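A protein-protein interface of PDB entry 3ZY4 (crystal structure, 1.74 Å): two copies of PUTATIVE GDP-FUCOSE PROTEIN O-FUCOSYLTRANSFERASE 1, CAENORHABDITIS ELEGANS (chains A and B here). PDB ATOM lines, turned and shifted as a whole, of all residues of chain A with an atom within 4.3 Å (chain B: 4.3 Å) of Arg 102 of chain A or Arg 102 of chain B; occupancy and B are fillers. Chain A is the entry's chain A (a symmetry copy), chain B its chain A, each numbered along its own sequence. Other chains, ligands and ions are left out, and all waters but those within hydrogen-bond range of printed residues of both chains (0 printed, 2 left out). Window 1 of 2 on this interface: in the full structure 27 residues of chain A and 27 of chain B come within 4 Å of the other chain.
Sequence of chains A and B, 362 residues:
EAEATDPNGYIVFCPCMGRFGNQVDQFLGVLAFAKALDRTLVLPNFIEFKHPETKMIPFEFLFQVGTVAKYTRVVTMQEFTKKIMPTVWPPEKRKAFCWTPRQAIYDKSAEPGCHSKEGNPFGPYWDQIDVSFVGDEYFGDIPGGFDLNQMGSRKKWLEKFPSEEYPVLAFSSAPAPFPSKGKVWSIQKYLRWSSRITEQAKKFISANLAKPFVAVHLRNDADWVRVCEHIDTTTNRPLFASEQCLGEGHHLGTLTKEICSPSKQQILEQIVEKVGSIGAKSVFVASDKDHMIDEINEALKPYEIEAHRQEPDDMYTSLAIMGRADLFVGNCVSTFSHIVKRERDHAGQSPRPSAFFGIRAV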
ATOM      1  N   MET A  17       5.824  19.684 -19.582  1.00  0.00           N
ATOM      2  CA  MET A  17       4.760  20.413 -20.283  1.00  0.00           C
ATOM      3  C   MET A  17       4.673  21.850 -19.791  1.00  0.00           C
ATOM      4  O   MET A  17       4.369  22.102 -18.640  1.00  0.00           O
ATOM      5  CB  MET A  17       3.388  19.738 -20.129  1.00  0.00           C
ATOM      6  CG  MET A  17       2.213  20.636 -20.601  1.00  0.00           C
ATOM      7  SD  MET A  17       0.629  19.811 -20.467  1.00  0.00           S
ATOM      8  CE  MET A  17       1.082  18.722 -21.738  1.00  0.00           C
ATOM      9  N   THR A 100       1.057   4.974 -24.108  1.00  0.00           N
ATOM     10  CA  THR A 100       0.980   4.136 -25.284  1.00  0.00           C
ATOM     11  C   THR A 100       2.245   4.333 -26.134  1.00  0.00           C
ATOM     12  O   THR A 100       2.871   5.386 -26.035  1.00  0.00           O
ATOM     13  CB  THR A 100      -0.306   4.511 -26.100  1.00  0.00           C
ATOM     14  OG1 THR A 100      -0.663   3.441 -26.971  1.00  0.00           O
ATOM     15  CG2 THR A 100      -0.181   5.828 -26.872  1.00  0.00           C
ATOM     16  N   PRO A 101       2.620   3.332 -26.970  1.00  0.00           N
ATOM     17  CA  PRO A 101       3.742   3.640 -27.878  1.00  0.00           C
ATOM     18  C   PRO A 101       3.388   4.694 -28.929  1.00  0.00           C
ATOM     19  O   PRO A 101       2.261   4.704 -29.486  1.00  0.00           O
ATOM     20  CB  PRO A 101       4.001   2.302 -28.577  1.00  0.00           C
ATOM     21  CG  PRO A 101       2.713   1.499 -28.416  1.00  0.00           C
ATOM     22  CD  PRO A 101       2.229   1.908 -27.040  1.00  0.00           C
ATOM     23  N   ARG A 102       4.369   5.535 -29.251  1.00  0.00           N
ATOM     24  CA  ARG A 102       4.160   6.579 -30.250  1.00  0.00           C
ATOM     25  C   ARG A 102       5.280   6.572 -31.272  1.00  0.00           C
ATOM     26  O   ARG A 102       6.374   6.005 -31.052  1.00  0.00           O
ATOM     27  CB  ARG A 102       4.041   7.952 -29.584  1.00  0.00           C
ATOM     28  CG  ARG A 102       2.861   8.013 -28.576  1.00  0.00           C
ATOM     29  CD  ARG A 102       2.697   9.350 -27.885  1.00  0.00           C
ATOM     30  NE  ARG A 102       2.034  10.377 -28.684  1.00  0.00           N
ATOM     31  CZ  ARG A 102       2.700  11.303 -29.356  1.00  0.00           C
ATOM     32  NH1 ARG A 102       4.023  11.288 -29.317  1.00  0.00           N
ATOM     33  NH2 ARG A 102       2.066  12.228 -30.055  1.00  0.00           N
ATOM     34  N   GLN A 103       4.973   7.172 -32.412  1.00  0.00           N
ATOM     35  CA  GLN A 103       5.943   7.406 -33.488  1.00  0.00           C
ATOM     36  C   GLN A 103       6.865   8.613 -33.202  1.00  0.00           C
ATOM     37  O   GLN A 103       6.392   9.748 -32.961  1.00  0.00           O
ATOM     38  CB  GLN A 103       5.179   7.655 -34.774  1.00  0.00           C
ATOM     39  CG  GLN A 103       6.065   8.042 -35.941  1.00  0.00           C
ATOM     40  CD  GLN A 103       7.054   6.953 -36.275  1.00  0.00           C
ATOM     41  OE1 GLN A 103       6.672   5.823 -36.556  1.00  0.00           O
ATOM     42  NE2 GLN A 103       8.344   7.301 -36.291  1.00  0.00           N
ATOM     43  N   ALA A 104       8.176   8.368 -33.207  1.00  0.00           N
ATOM     44  CA  ALA A 104       9.152   9.474 -33.113  1.00  0.00           C
ATOM     45  C   ALA A 104       8.975  10.500 -34.251  1.00  0.00           C
ATOM     46  O   ALA A 104       8.733  10.144 -35.408  1.00  0.00           O
ATOM     47  CB  ALA A 104      10.583   8.918 -33.137  1.00  0.00           C
ATOM     48  N   PRO A 112       8.838   2.195 -32.051  1.00  0.00           N
ATOM     49  CA  PRO A 112       7.706   2.785 -31.296  1.00  0.00           C
ATOM     50  C   PRO A 112       7.938   2.800 -29.787  1.00  0.00           C
ATOM     51  O   PRO A 112       8.434   1.815 -29.203  1.00  0.00           O
ATOM     52  CB  PRO A 112       6.513   1.880 -31.647  1.00  0.00           C
ATOM     53  CG  PRO A 112       6.888   1.279 -33.022  1.00  0.00           C
ATOM     54  CD  PRO A 112       8.396   1.167 -33.018  1.00  0.00           C
ATOM     55  N   GLY A 113       7.626   3.925 -29.161  1.00  0.00           N
ATOM     56  CA  GLY A 113       7.898   4.040 -27.734  1.00  0.00           C
ATOM     57  C   GLY A 113       7.417   5.320 -27.125  1.00  0.00           C
ATOM     58  O   GLY A 113       6.590   6.025 -27.705  1.00  0.00           O
ATOM     59  N   HIS A 115       9.554   7.794 -26.298  1.00  0.00           N
ATOM     60  CA  HIS A 115      10.469   8.852 -26.766  1.00  0.00           C
ATOM     61  C   HIS A 115      10.673   9.927 -25.723  1.00  0.00           C
ATOM     62  O   HIS A 115      10.535  11.122 -25.986  1.00  0.00           O
ATOM     63  CB  HIS A 115      10.036   9.400 -28.149  1.00  0.00           C
ATOM     64  CG  HIS A 115       9.852   8.306 -29.132  1.00  0.00           C
ATOM     65  ND1 HIS A 115      10.914   7.566 -29.616  1.00  0.00           N
ATOM     66  CD2 HIS A 115       8.730   7.754 -29.654  1.00  0.00           C
ATOM     67  CE1 HIS A 115      10.448   6.629 -30.423  1.00  0.00           C
ATOM     68  NE2 HIS A 115       9.126   6.711 -30.441  1.00  0.00           N
ATOM     69  N   MET B  17       2.084   5.498 -37.432  1.00  0.00           N
ATOM     70  CA  MET B  17       3.180   4.792 -36.757  1.00  0.00           C
ATOM     71  C   MET B  17       3.801   3.752 -37.675  1.00  0.00           C
ATOM     72  O   MET B  17       3.157   2.797 -38.069  1.00  0.00           O
ATOM     73  CB  MET B  17       2.726   4.116 -35.453  1.00  0.00           C
ATOM     74  CG  MET B  17       3.778   3.127 -34.884  1.00  0.00           C
ATOM     75  SD  MET B  17       3.256   2.392 -33.337  1.00  0.00           S
ATOM     76  CE  MET B  17       3.407   3.929 -32.549  1.00  0.00           C
ATOM     77  N   THR B 100      -4.176  12.044 -24.108  1.00  0.00           N
ATOM     78  CA  THR B 100      -3.879  13.045 -23.108  1.00  0.00           C
ATOM     79  C   THR B 100      -3.231  14.264 -23.784  1.00  0.00           C
ATOM     80  O   THR B 100      -2.644  14.110 -24.851  1.00  0.00           O
ATOM     81  CB  THR B 100      -2.919  12.428 -22.030  1.00  0.00           C
ATOM     82  OG1 THR B 100      -2.979  13.190 -20.828  1.00  0.00           O
ATOM     83  CG2 THR B 100      -1.474  12.274 -22.512  1.00  0.00           C
ATOM     84  N   PRO B 101      -3.331  15.469 -23.167  1.00  0.00           N
ATOM     85  CA  PRO B 101      -2.554  16.567 -23.775  1.00  0.00           C
ATOM     86  C   PRO B 101      -1.042  16.370 -23.648  1.00  0.00           C
ATOM     87  O   PRO B 101      -0.533  15.902 -22.597  1.00  0.00           O
ATOM     88  CB  PRO B 101      -2.971  17.787 -22.949  1.00  0.00           C
ATOM     89  CG  PRO B 101      -3.525  17.227 -21.640  1.00  0.00           C
ATOM     90  CD  PRO B 101      -4.212  15.951 -22.082  1.00  0.00           C
ATOM     91  N   ARG B 102      -0.319  16.790 -24.684  1.00  0.00           N
ATOM     92  CA  ARG B 102       1.135  16.668 -24.679  1.00  0.00           C
ATOM     93  C   ARG B 102       1.782  17.984 -25.067  1.00  0.00           C
ATOM     94  O   ARG B 102       1.145  18.889 -25.652  1.00  0.00           O
ATOM     95  CB  ARG B 102       1.589  15.544 -25.613  1.00  0.00           C
ATOM     96  CG  ARG B 102       0.994  14.168 -25.205  1.00  0.00           C
ATOM     97  CD  ARG B 102       1.409  13.017 -26.097  1.00  0.00           C
ATOM     98  NE  ARG B 102       2.745  12.488 -25.833  1.00  0.00           N
ATOM     99  CZ  ARG B 102       3.807  12.842 -26.541  1.00  0.00           C
ATOM    100  NH1 ARG B 102       3.657  13.725 -27.515  1.00  0.00           N
ATOM    101  NH2 ARG B 102       4.998  12.329 -26.287  1.00  0.00           N
ATOM    102  N   GLN B 103       3.048  18.093 -24.692  1.00  0.00           N
ATOM    103  CA  GLN B 103       3.910  19.216 -25.079  1.00  0.00           C
ATOM    104  C   GLN B 103       4.442  19.084 -26.524  1.00  0.00           C
ATOM    105  O   GLN B 103       5.075  18.068 -26.892  1.00  0.00           O
ATOM    106  CB  GLN B 103       5.083  19.270 -24.118  1.00  0.00           C
ATOM    107  CG  GLN B 103       6.122  20.308 -24.488  1.00  0.00           C
ATOM    108  CD  GLN B 103       5.545  21.701 -24.482  1.00  0.00           C
ATOM    109  OE1 GLN B 103       5.016  22.157 -23.475  1.00  0.00           O
ATOM    110  NE2 GLN B 103       5.683  22.411 -25.607  1.00  0.00           N
ATOM    111  N   ALA B 104       4.168  20.098 -27.347  1.00  0.00           N
ATOM    112  CA  ALA B 104       4.766  20.157 -28.697  1.00  0.00           C
ATOM    113  C   ALA B 104       6.308  20.142 -28.648  1.00  0.00           C
ATOM    114  O   ALA B 104       6.932  20.781 -27.796  1.00  0.00           O
ATOM    115  CB  ALA B 104       4.286  21.417 -29.432  1.00  0.00           C
ATOM    116  N   PRO B 112      -0.915  22.997 -24.974  1.00  0.00           N
ATOM    117  CA  PRO B 112      -0.972  21.527 -24.782  1.00  0.00           C
ATOM    118  C   PRO B 112      -2.083  20.862 -25.589  1.00  0.00           C
ATOM    119  O   PRO B 112      -3.220  21.372 -25.662  1.00  0.00           O
ATOM    120  CB  PRO B 112      -1.227  21.360 -23.274  1.00  0.00           C
ATOM    121  CG  PRO B 112      -0.662  22.657 -22.650  1.00  0.00           C
ATOM    122  CD  PRO B 112      -0.869  23.733 -23.692  1.00  0.00           C
ATOM    123  N   GLY B 113      -1.752  19.751 -26.230  1.00  0.00           N
ATOM    124  CA  GLY B 113      -2.740  19.106 -27.086  1.00  0.00           C
ATOM    125  C   GLY B 113      -2.276  17.814 -27.682  1.00  0.00           C
ATOM    126  O   GLY B 113      -1.305  17.215 -27.217  1.00  0.00           O
ATOM    127  N   HIS B 115      -1.384  17.581 -30.925  1.00  0.00           N
ATOM    128  CA  HIS B 115      -0.402  17.928 -31.971  1.00  0.00           C
ATOM    129  C   HIS B 115      -0.453  16.966 -33.136  1.00  0.00           C
ATOM    130  O   HIS B 115       0.561  16.419 -33.571  1.00  0.00           O
ATOM    131  CB  HIS B 115       1.016  18.109 -31.374  1.00  0.00           C
ATOM    132  CG  HIS B 115       1.008  19.061 -30.237  1.00  0.00           C
ATOM    133  ND1 HIS B 115       0.770  20.411 -30.411  1.00  0.00           N
ATOM    134  CD2 HIS B 115       1.110  18.858 -28.902  1.00  0.00           C
ATOM    135  CE1 HIS B 115       0.764  20.999 -29.228  1.00  0.00           C
ATOM    136  NE2 HIS B 115       0.944  20.071 -28.299  1.00  0.00           N
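The guanidinium group (NH1) of Arg 102 of chain B lies close to the guanidinium group (NH1) of Arg 102 of chain A, 3.1 Å away.
N of Arg 102 of chain B sits at hydrogen-bond distance from O of Gly 113 of chain B (2.8 Å).
The backbone carbonyl oxygen of Arg 102 of chain B sits at hydrogen-bond distance from a ring nitrogen (NE2) of His 115 of chain B (2.9 Å).
N of Arg 102 of chain A sits at hydrogen-bond distance from O of Gly 113 of chain A, at 2.8 Å.
The backbone carbonyl oxygen (O) of Arg 102 of chain A is in hydrogen-bond range of a ring nitrogen (NE2) of His 115 of chain A (2.9 Å).
Among the printed residues, merely in contact across the chains: Pro 101 of chain A with Met 17 of chain B, Met 17 of chain A with Pro 101 of chain B, Met 17 of chain A with Arg 102 of chain B, Arg 102 of chain A with Met 17 of chain B, Met 17 of chain A with Gln 103 of chain B, Gln 103 of chain A with Met 17 of chain B, Met 17 of chain A with Pro 112 of chain B and Pro 112 of chain A with Met 17 of chain B.
Of the printed residues of chain B, Pro 101 of chain A touches Met 17.
Arg 102 of chain A touches two residues of chain B.
Printed residues of chain A within 4 Å of Pro 101 of chain B: Met 17 (3.4 Å).
Printed residues of chain A within 4 Å of Gln 103 of chain B: Met 17 (3.6 Å).
Printed residues of chain A within 4 Å of Pro 112 of chain B: Met 17.
The nearest printed residue of chain B that does not touch Arg 102 of chain A is His 115 of chain B (5.7 Å).
The nearest printed residue of chain A that does not touch Arg 102 of chain B is His 115 of chain A (5.7 Å).
Hydrophobic or aromatic side chains of chain B within 4 Å of the printed part of chain A: Met 17 and Pro 112.
Along chain B the printed residues that touch a printed residue of chain A span positions 17 to 112.
Of the 9 printed residues of chain A, 5 touch a printed residue of chain B.
Printed residues of chain A that touch a printed residue of chain B: Met 17, Pro 101, Arg 102, Gln 103 and Pro 112.
Among the printed residues, no Asp or Glu carboxylate lies within 4 Å of a Lys or Arg side-chain nitrogen of the other chain.
Met 17 of chain A touches Pro 101 of chain B, and with the chains exchanged Pro 101 of chain A touches Met 17 of chain B.
Met 17 of chain A touches Arg 102 of chain B, and with the chains exchanged Arg 102 of chain A touches Met 17 of chain B.
Met 17 of chain A touches Pro 112 of chain B, and with the chains exchanged Pro 112 of chain A touches Met 17 of chain B.
Arg 102 of chain B touches its own counterpart, Arg 102 of chain A.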
